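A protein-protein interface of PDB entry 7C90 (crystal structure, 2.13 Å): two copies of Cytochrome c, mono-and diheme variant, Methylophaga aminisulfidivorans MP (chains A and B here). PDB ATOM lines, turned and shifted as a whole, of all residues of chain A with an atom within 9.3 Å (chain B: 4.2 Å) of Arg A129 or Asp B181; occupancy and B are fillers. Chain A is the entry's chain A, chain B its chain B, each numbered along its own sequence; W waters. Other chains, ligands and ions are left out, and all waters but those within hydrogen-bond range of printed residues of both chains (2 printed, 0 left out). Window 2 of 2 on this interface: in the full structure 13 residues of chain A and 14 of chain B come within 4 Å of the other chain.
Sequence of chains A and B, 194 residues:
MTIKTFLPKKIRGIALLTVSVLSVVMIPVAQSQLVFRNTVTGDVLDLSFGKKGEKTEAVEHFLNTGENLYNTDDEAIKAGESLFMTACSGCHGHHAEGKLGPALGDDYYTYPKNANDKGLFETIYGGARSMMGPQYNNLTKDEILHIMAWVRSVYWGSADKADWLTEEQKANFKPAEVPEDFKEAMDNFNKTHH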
ATOM      1  N   ASN A  38      10.400  10.523  -9.023  1.00  0.00           N
ATOM      2  CA  ASN A  38      10.443  10.856 -10.459  1.00  0.00           C
ATOM      3  C   ASN A  38      11.710  10.244 -11.096  1.00  0.00           C
ATOM      4  O   ASN A  38      12.818  10.403 -10.573  1.00  0.00           O
ATOM      5  CB  ASN A  38      10.318  12.361 -10.634  1.00  0.00           C
ATOM      6  CG  ASN A  38      10.251  12.746 -12.092  1.00  0.00           C
ATOM      7  OD1 ASN A  38      11.245  12.630 -12.801  1.00  0.00           O
ATOM      8  ND2 ASN A  38       9.078  13.165 -12.546  1.00  0.00           N
ATOM      9  N   THR A  39      11.532   9.568 -12.220  1.00  0.00           N
ATOM     10  CA  THR A  39      12.567   8.786 -12.927  1.00  0.00           C
ATOM     11  C   THR A  39      13.703   9.701 -13.425  1.00  0.00           C
ATOM     12  O   THR A  39      14.854   9.245 -13.470  1.00  0.00           O
ATOM     13  CB  THR A  39      11.865   8.014 -14.051  1.00  0.00           C
ATOM     14  OG1 THR A  39      10.961   7.128 -13.389  1.00  0.00           O
ATOM     15  CG2 THR A  39      12.852   7.296 -14.939  1.00  0.00           C
ATOM     16  N   VAL A  40      13.387  10.945 -13.794  1.00  0.00           N
ATOM     17  CA  VAL A  40      14.346  11.922 -14.392  1.00  0.00           C
ATOM     18  C   VAL A  40      14.843  12.896 -13.306  1.00  0.00           C
ATOM     19  O   VAL A  40      16.069  13.075 -13.191  1.00  0.00           O
ATOM     20  CB  VAL A  40      13.698  12.662 -15.578  1.00  0.00           C
ATOM     21  CG1 VAL A  40      14.549  13.828 -16.060  1.00  0.00           C
ATOM     22  CG2 VAL A  40      13.384  11.708 -16.715  1.00  0.00           C
ATOM     23  N   THR A  41      13.940  13.508 -12.542  1.00  0.00           N
ATOM     24  CA  THR A  41      14.274  14.635 -11.632  1.00  0.00           C
ATOM     25  C   THR A  41      14.680  14.117 -10.255  1.00  0.00           C
ATOM     26  O   THR A  41      15.301  14.871  -9.569  1.00  0.00           O
ATOM     27  CB  THR A  41      13.102  15.592 -11.422  1.00  0.00           C
ATOM     28  OG1 THR A  41      12.086  14.861 -10.721  1.00  0.00           O
ATOM     29  CG2 THR A  41      12.583  16.182 -12.710  1.00  0.00           C
ATOM     30  N   GLY A  42      14.322  12.893  -9.859  1.00  0.00           N
ATOM     31  CA  GLY A  42      14.550  12.414  -8.486  1.00  0.00           C
ATOM     32  C   GLY A  42      13.605  13.087  -7.485  1.00  0.00           C
ATOM     33  O   GLY A  42      13.625  12.703  -6.337  1.00  0.00           O
ATOM     34  N   HIS A  92       4.745   3.409 -28.265  1.00  0.00           N
ATOM     35  CA  HIS A  92       5.538   2.206 -27.879  1.00  0.00           C
ATOM     36  C   HIS A  92       5.242   0.991 -28.793  1.00  0.00           C
ATOM     37  O   HIS A  92       5.916  -0.035 -28.647  1.00  0.00           O
ATOM     38  CB  HIS A  92       5.317   1.929 -26.387  1.00  0.00           C
ATOM     39  CG  HIS A  92       5.996   2.916 -25.488  1.00  0.00           C
ATOM     40  ND1 HIS A  92       7.336   2.845 -25.239  1.00  0.00           N
ATOM     41  CD2 HIS A  92       5.516   3.957 -24.755  1.00  0.00           C
ATOM     42  CE1 HIS A  92       7.676   3.803 -24.387  1.00  0.00           C
ATOM     43  NE2 HIS A  92       6.564   4.531 -24.059  1.00  0.00           N
ATOM     44  N   LEU A 100       8.312   5.342 -31.345  1.00  0.00           N
ATOM     45  CA  LEU A 100       8.916   6.647 -30.956  1.00  0.00           C
ATOM     46  C   LEU A 100       9.656   6.480 -29.627  1.00  0.00           C
ATOM     47  O   LEU A 100      10.794   6.938 -29.507  1.00  0.00           O
ATOM     48  CB  LEU A 100       7.816   7.708 -30.819  1.00  0.00           C
ATOM     49  CG  LEU A 100       8.323   9.096 -30.420  1.00  0.00           C
ATOM     50  CD1 LEU A 100       8.188  10.074 -31.562  1.00  0.00           C
ATOM     51  CD2 LEU A 100       7.579   9.614 -29.208  1.00  0.00           C
ATOM     52  N   GLY A 101       8.989   5.876 -28.651  1.00  0.00           N
ATOM     53  CA  GLY A 101       9.590   5.451 -27.382  1.00  0.00           C
ATOM     54  C   GLY A 101      10.163   4.043 -27.528  1.00  0.00           C
ATOM     55  O   GLY A 101       9.957   3.361 -28.535  1.00  0.00           O
ATOM     56  N   PRO A 102      10.932   3.583 -26.534  1.00  0.00           N
ATOM     57  CA  PRO A 102      11.510   2.244 -26.592  1.00  0.00           C
ATOM     58  C   PRO A 102      10.549   1.042 -26.536  1.00  0.00           C
ATOM     59  O   PRO A 102       9.364   1.120 -26.240  1.00  0.00           O
ATOM     60  CB  PRO A 102      12.478   2.239 -25.403  1.00  0.00           C
ATOM     61  CG  PRO A 102      11.985   3.344 -24.475  1.00  0.00           C
ATOM     62  CD  PRO A 102      11.386   4.383 -25.390  1.00  0.00           C
ATOM     63  N   THR A 110      16.274   1.971 -20.686  1.00  0.00           N
ATOM     64  CA  THR A 110      16.805   3.337 -20.568  1.00  0.00           C
ATOM     65  C   THR A 110      17.119   3.627 -19.092  1.00  0.00           C
ATOM     66  O   THR A 110      18.204   4.179 -18.799  1.00  0.00           O
ATOM     67  CB  THR A 110      15.822   4.320 -21.199  1.00  0.00           C
ATOM     68  OG1 THR A 110      15.466   3.744 -22.455  1.00  0.00           O
ATOM     69  CG2 THR A 110      16.397   5.710 -21.302  1.00  0.00           C
ATOM     70  N   TYR A 111      16.191   3.288 -18.198  1.00  0.00           N
ATOM     71  CA  TYR A 111      16.304   3.467 -16.737  1.00  0.00           C
ATOM     72  C   TYR A 111      16.227   2.096 -16.082  1.00  0.00           C
ATOM     73  O   TYR A 111      15.215   1.411 -16.173  1.00  0.00           O
ATOM     74  CB  TYR A 111      15.232   4.448 -16.272  1.00  0.00           C
ATOM     75  CG  TYR A 111      15.164   5.737 -17.058  1.00  0.00           C
ATOM     76  CD1 TYR A 111      16.050   6.770 -16.802  1.00  0.00           C
ATOM     77  CD2 TYR A 111      14.227   5.928 -18.052  1.00  0.00           C
ATOM     78  CE1 TYR A 111      16.006   7.956 -17.519  1.00  0.00           C
ATOM     79  CE2 TYR A 111      14.154   7.118 -18.760  1.00  0.00           C
ATOM     80  CZ  TYR A 111      15.036   8.143 -18.481  1.00  0.00           C
ATOM     81  OH  TYR A 111      15.001   9.301 -19.203  1.00  0.00           O
ATOM     82  N   THR A 123       7.841   5.650 -13.459  1.00  0.00           N
ATOM     83  CA  THR A 123       8.131   6.167 -14.812  1.00  0.00           C
ATOM     84  C   THR A 123       6.776   6.517 -15.447  1.00  0.00           C
ATOM     85  O   THR A 123       6.640   7.584 -16.060  1.00  0.00           O
ATOM     86  CB  THR A 123       8.988   5.178 -15.606  1.00  0.00           C
ATOM     87  OG1 THR A 123      10.268   5.040 -15.000  1.00  0.00           O
ATOM     88  CG2 THR A 123       9.140   5.587 -17.055  1.00  0.00           C
ATOM     89  N   GLY A 126       4.854   9.529 -13.105  1.00  0.00           N
ATOM     90  CA  GLY A 126       5.605  10.804 -13.046  1.00  0.00           C
ATOM     91  C   GLY A 126       6.210  11.207 -14.379  1.00  0.00           C
ATOM     92  O   GLY A 126       6.630  12.332 -14.493  1.00  0.00           O
ATOM     93  N   GLY A 127       6.224  10.321 -15.369  1.00  0.00           N
ATOM     94  CA  GLY A 127       6.790  10.603 -16.692  1.00  0.00           C
ATOM     95  C   GLY A 127       8.309  10.527 -16.681  1.00  0.00           C
ATOM     96  O   GLY A 127       8.900  10.232 -15.663  1.00  0.00           O
ATOM     97  N   ALA A 128       8.910  10.723 -17.822  1.00  0.00           N
ATOM     98  CA  ALA A 128      10.376  10.730 -18.004  1.00  0.00           C
ATOM     99  C   ALA A 128      10.699  11.956 -18.853  1.00  0.00           C
ATOM    100  O   ALA A 128      10.089  12.997 -18.562  1.00  0.00           O
ATOM    101  CB  ALA A 128      10.827   9.405 -18.594  1.00  0.00           C
ATOM    102  N   ARG A 129      11.610  11.860 -19.826  1.00  0.00           N
ATOM    103  CA  ARG A 129      12.061  13.006 -20.655  1.00  0.00           C
ATOM    104  C   ARG A 129      11.116  13.173 -21.842  1.00  0.00           C
ATOM    105  O   ARG A 129      10.401  12.210 -22.180  1.00  0.00           O
ATOM    106  CB  ARG A 129      13.459  12.774 -21.248  1.00  0.00           C
ATOM    107  CG  ARG A 129      14.592  12.895 -20.243  1.00  0.00           C
ATOM    108  CD  ARG A 129      15.950  12.790 -20.914  1.00  0.00           C
ATOM    109  NE  ARG A 129      16.755  11.952 -20.049  1.00  0.00           N
ATOM    110  CZ  ARG A 129      17.292  12.355 -18.910  1.00  0.00           C
ATOM    111  NH1 ARG A 129      17.158  13.610 -18.520  1.00  0.00           N
ATOM    112  NH2 ARG A 129      17.993  11.505 -18.185  1.00  0.00           N
ATOM    113  N   SER A 130      11.179  14.335 -22.475  1.00  0.00           N
ATOM    114  CA  SER A 130      10.682  14.576 -23.853  1.00  0.00           C
ATOM    115  C   SER A 130       9.197  14.197 -23.906  1.00  0.00           C
ATOM    116  O   SER A 130       8.472  14.586 -22.992  1.00  0.00           O
ATOM    117  CB  SER A 130      11.553  13.813 -24.841  1.00  0.00           C
ATOM    118  OG  SER A 130      11.342  14.253 -26.179  1.00  0.00           O
ATOM    119  N   MET A 131       8.817  13.377 -24.875  1.00  0.00           N
ATOM    120  CA  MET A 131       7.413  12.978 -25.124  1.00  0.00           C
ATOM    121  C   MET A 131       6.884  11.972 -24.097  1.00  0.00           C
ATOM    122  O   MET A 131       5.768  11.569 -24.244  1.00  0.00           O
ATOM    123  CB  MET A 131       7.311  12.348 -26.509  1.00  0.00           C
ATOM    124  CG  MET A 131       8.140  13.046 -27.530  1.00  0.00           C
ATOM    125  SD  MET A 131       7.191  14.395 -28.168  1.00  0.00           S
ATOM    126  CE  MET A 131       5.788  13.495 -28.806  1.00  0.00           C
ATOM    127  N   MET A 132       7.681  11.533 -23.138  1.00  0.00           N
ATOM    128  CA  MET A 132       7.143  10.569 -22.152  1.00  0.00           C
ATOM    129  C   MET A 132       6.590  11.392 -20.991  1.00  0.00           C
ATOM    130  O   MET A 132       7.290  11.622 -20.041  1.00  0.00           O
ATOM    131  CB  MET A 132       8.217   9.582 -21.696  1.00  0.00           C
ATOM    132  CG  MET A 132       7.727   8.436 -20.844  1.00  0.00           C
ATOM    133  SD  MET A 132       6.242   7.592 -21.341  1.00  0.00           S
ATOM    134  CE  MET A 132       5.748   6.979 -19.746  1.00  0.00           C
ATOM    135  N   GLY A 133       5.370  11.878 -21.160  1.00  0.00           N
ATOM    136  CA  GLY A 133       4.726  12.728 -20.154  1.00  0.00           C
ATOM    137  C   GLY A 133       4.208  11.953 -18.960  1.00  0.00           C
ATOM    138  O   GLY A 133       4.014  10.777 -19.058  1.00  0.00           O
ATOM    139  N   PRO A 134       3.981  12.598 -17.806  1.00  0.00           N
ATOM    140  CA  PRO A 134       3.398  11.911 -16.670  1.00  0.00           C
ATOM    141  C   PRO A 134       1.947  11.524 -17.009  1.00  0.00           C
ATOM    142  O   PRO A 134       1.291  12.248 -17.676  1.00  0.00           O
ATOM    143  CB  PRO A 134       3.490  12.950 -15.556  1.00  0.00           C
ATOM    144  CG  PRO A 134       3.509  14.257 -16.274  1.00  0.00           C
ATOM    145  CD  PRO A 134       4.286  13.986 -17.535  1.00  0.00           C
ATOM    146  N   HIS B  95      23.541  18.829 -24.264  1.00  0.00           N
ATOM    147  CA  HIS B  95      24.594  18.476 -23.262  1.00  0.00           C
ATOM    148  C   HIS B  95      24.701  16.963 -23.073  1.00  0.00           C
ATOM    149  O   HIS B  95      25.350  16.508 -22.091  1.00  0.00           O
ATOM    150  CB  HIS B  95      24.366  19.260 -21.950  1.00  0.00           C
ATOM    151  CG  HIS B  95      24.268  20.727 -22.180  1.00  0.00           C
ATOM    152  ND1 HIS B  95      23.099  21.325 -22.665  1.00  0.00           N
ATOM    153  CD2 HIS B  95      25.180  21.715 -22.053  1.00  0.00           C
ATOM    154  CE1 HIS B  95      23.294  22.622 -22.805  1.00  0.00           C
ATOM    155  NE2 HIS B  95      24.559  22.891 -22.439  1.00  0.00           N
ATOM    156  N   GLU B  97      22.514  14.932 -22.310  1.00  0.00           N
ATOM    157  CA  GLU B  97      21.768  14.684 -21.047  1.00  0.00           C
ATOM    158  C   GLU B  97      20.539  13.812 -21.341  1.00  0.00           C
ATOM    159  O   GLU B  97      19.816  13.441 -20.401  1.00  0.00           O
ATOM    160  CB  GLU B  97      21.414  16.037 -20.417  1.00  0.00           C
ATOM    161  CG  GLU B  97      20.241  16.755 -21.078  1.00  0.00           C
ATOM    162  CD  GLU B  97      20.512  17.633 -22.299  1.00  0.00           C
ATOM    163  OE1 GLU B  97      21.637  17.575 -22.852  1.00  0.00           O
ATOM    164  OE2 GLU B  97      19.567  18.367 -22.729  1.00  0.00           O
ATOM    165  N   GLY B  98      20.288  13.492 -22.609  1.00  0.00           N
ATOM    166  CA  GLY B  98      19.067  12.762 -22.996  1.00  0.00           C
ATOM    167  C   GLY B  98      17.955  13.709 -23.407  1.00  0.00           C
ATOM    168  O   GLY B  98      17.892  14.838 -22.893  1.00  0.00           O
ATOM    169  N   LYS B  99      17.111  13.252 -24.321  1.00  0.00           N
ATOM    170  CA  LYS B  99      15.834  13.911 -24.697  1.00  0.00           C
ATOM    171  C   LYS B  99      14.869  12.807 -25.162  1.00  0.00           C
ATOM    172  O   LYS B  99      14.262  12.190 -24.306  1.00  0.00           O
ATOM    173  CB  LYS B  99      16.101  15.008 -25.729  1.00  0.00           C
ATOM    174  CG  LYS B  99      14.959  15.991 -25.887  1.00  0.00           C
ATOM    175  CD  LYS B  99      14.981  16.738 -27.188  1.00  0.00           C
ATOM    176  CE  LYS B  99      15.451  18.165 -27.051  1.00  0.00           C
ATOM    177  NZ  LYS B  99      15.070  18.969 -28.238  1.00  0.00           N
ATOM    178  N   PRO B 179      25.207  18.495 -16.471  1.00  0.00           N
ATOM    179  CA  PRO B 179      24.391  19.590 -16.971  1.00  0.00           C
ATOM    180  C   PRO B 179      23.022  19.590 -16.270  1.00  0.00           C
ATOM    181  O   PRO B 179      22.495  18.517 -15.922  1.00  0.00           O
ATOM    182  CB  PRO B 179      24.280  19.284 -18.473  1.00  0.00           C
ATOM    183  CG  PRO B 179      24.389  17.781 -18.522  1.00  0.00           C
ATOM    184  CD  PRO B 179      25.446  17.462 -17.491  1.00  0.00           C
ATOM    185  N   GLU B 180      22.493  20.790 -16.053  1.00  0.00           N
ATOM    186  CA  GLU B 180      21.185  21.066 -15.400  1.00  0.00           C
ATOM    187  C   GLU B 180      20.069  20.260 -16.081  1.00  0.00           C
ATOM    188  O   GLU B 180      19.155  19.808 -15.366  1.00  0.00           O
ATOM    189  CB  GLU B 180      20.873  22.560 -15.523  1.00  0.00           C
ATOM    190  CG  GLU B 180      19.637  23.019 -14.772  1.00  0.00           C
ATOM    191  CD  GLU B 180      19.465  24.536 -14.808  1.00  0.00           C
ATOM    192  OE1 GLU B 180      19.832  25.159 -15.845  1.00  0.00           O
ATOM    193  OE2 GLU B 180      19.000  25.100 -13.791  1.00  0.00           O
ATOM    194  N   ASP B 181      20.122  20.132 -17.410  1.00  0.00           N
ATOM    195  CA  ASP B 181      19.022  19.558 -18.230  1.00  0.00           C
ATOM    196  C   ASP B 181      18.910  18.051 -17.943  1.00  0.00           C
ATOM    197  O   ASP B 181      17.820  17.525 -18.165  1.00  0.00           O
ATOM    198  CB  ASP B 181      19.209  19.843 -19.722  1.00  0.00           C
ATOM    199  CG  ASP B 181      19.630  21.269 -20.075  1.00  0.00           C
ATOM    200  OD1 ASP B 181      20.824  21.603 -19.849  1.00  0.00           O
ATOM    201  OD2 ASP B 181      18.782  22.024 -20.610  1.00  0.00           O
ATOM    202  N   PHE B 182      19.968  17.395 -17.433  1.00  0.00           N
ATOM    203  CA  PHE B 182      19.944  15.959 -17.037  1.00  0.00           C
ATOM    204  C   PHE B 182      18.894  15.735 -15.933  1.00  0.00           C
ATOM    205  O   PHE B 182      18.246  14.658 -15.946  1.00  0.00           O
ATOM    206  CB  PHE B 182      21.323  15.494 -16.560  1.00  0.00           C
ATOM    207  CG  PHE B 182      21.416  14.025 -16.221  1.00  0.00           C
ATOM    208  CD1 PHE B 182      21.061  13.048 -17.144  1.00  0.00           C
ATOM    209  CD2 PHE B 182      21.872  13.618 -14.977  1.00  0.00           C
ATOM    210  CE1 PHE B 182      21.171  11.702 -16.836  1.00  0.00           C
ATOM    211  CE2 PHE B 182      21.974  12.268 -14.673  1.00  0.00           C
ATOM    212  CZ  PHE B 182      21.629  11.314 -15.603  1.00  0.00           C
ATOM    213  N   LYS B 183      18.794  16.712 -15.015  1.00  0.00           N
ATOM    214  CA  LYS B 183      17.867  16.827 -13.853  1.00  0.00           C
ATOM    215  C   LYS B 183      18.311  15.844 -12.764  1.00  0.00           C
ATOM    216  O   LYS B 183      19.108  16.195 -11.893  1.00  0.00           O
ATOM    217  CB  LYS B 183      16.405  16.677 -14.288  1.00  0.00           C
ATOM    218  CG  LYS B 183      15.867  17.820 -15.136  1.00  0.00           C
ATOM    219  CD  LYS B 183      14.418  17.671 -15.583  1.00  0.00           C
ATOM    220  CE  LYS B 183      14.250  17.255 -17.034  1.00  0.00           C
ATOM    221  NZ  LYS B 183      12.834  16.948 -17.348  1.00  0.00           N
HETATM  222  O   HOH W   1      18.169  12.211 -14.872  1.00  0.00           O
HETATM  223  O   HOH W   2      16.019  15.695 -19.389  1.00  0.00           O
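The guanidinium group of Arg A129 is in hydrogen-bond range of the backbone carbonyl oxygen of Phe B182 (3.0 Å).
O of Glu B97 sits close to NH1 of Arg A129 (3.3 Å).
The side-chain carboxylate (OE1) of Glu B97 sits at hydrogen-bond distance from the backbone NH (N) of His B95.
The side-chain hydroxyl of Tyr A111 is in hydrogen-bond range of the guanidinium group of Arg A129.
N of Val A40 lies within hydrogen-bond range of OD1 of Asn A38 (2.9 Å).
N of Thr A41 sits at hydrogen-bond distance from OD1 of Asn A38 (2.8 Å).
CG1 of Val A40 touches O of Phe B182, 3.8 Å away.
CE of Lys B183 touches CG1 of Val A40 (3.6 Å).
CD of Lys B183 touches CG2 of Thr A41, 3.7 Å away.
CD of Arg A129 touches C of Gly B98 (3.3 Å).
Lys B99 touches Arg A129 (O to CB, 3.2 Å).
Arg A129 touches Asp B181 (NH1 to O, 3.99 Å).
Ser A130 touches Lys B99.
Of the printed residues of chain B, Thr A41 touches Lys B183.
His A92 touches none of the printed residues of chain B.
Ala A128 touches none of the printed residues of chain B.
Of the printed residues of chain B, Arg A129 touches Glu B97 (3.1 Å), Gly B98 (3.3 Å), Lys B99 (3.2 Å), Asp B181 (3.99 Å) and Phe B182 (3.0 Å).
Of the printed residues of chain B, Ser A130 touches Lys B99 (3.2 Å).
Printed residues of chain A within 4 Å of Glu B97: Arg A129 (3.1 Å).
Gly B98 touches one residue of chain A.
Of the printed residues of chain A, Phe B182 touches Val A40 and Arg A129.
Of the printed residues of chain A, Lys B183 touches Val A40 and Thr A41.
The nearest printed residue of chain B that does not touch Arg A129 is Lys B183 (4.9 Å).
Hydrophobic or aromatic side chains of chain B that line the printed part of chain A: Phe B182.
Along chain B the printed residues that touch a printed residue of chain A span positions 97 to 183.
Along chain A the printed residues that touch a printed residue of chain B span positions 40 to 130.
Among the printed residues, no Asp or Glu carboxylate lies within 4 Å of a Lys or Arg side-chain nitrogen of the other chain.
No position is printed for both chains.
Of the 9 pairs that touch across the chains among the printed residues, none has its exchanged pair printed and touching as well.
Water W2 lies within hydrogen-bond range of the guanidinium group (NH1) of Arg A129 and the backbone carbonyl oxygen (O) of Asp B181.
Water W1 lies within hydrogen-bond range of the backbone carbonyl oxygen (O) of Phe B182 (2.7 Å), the backbone carbonyl oxygen (O) of Val A40 (2.8 Å) and the guanidinium group (NH2) of Arg A129 (3.4 Å).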
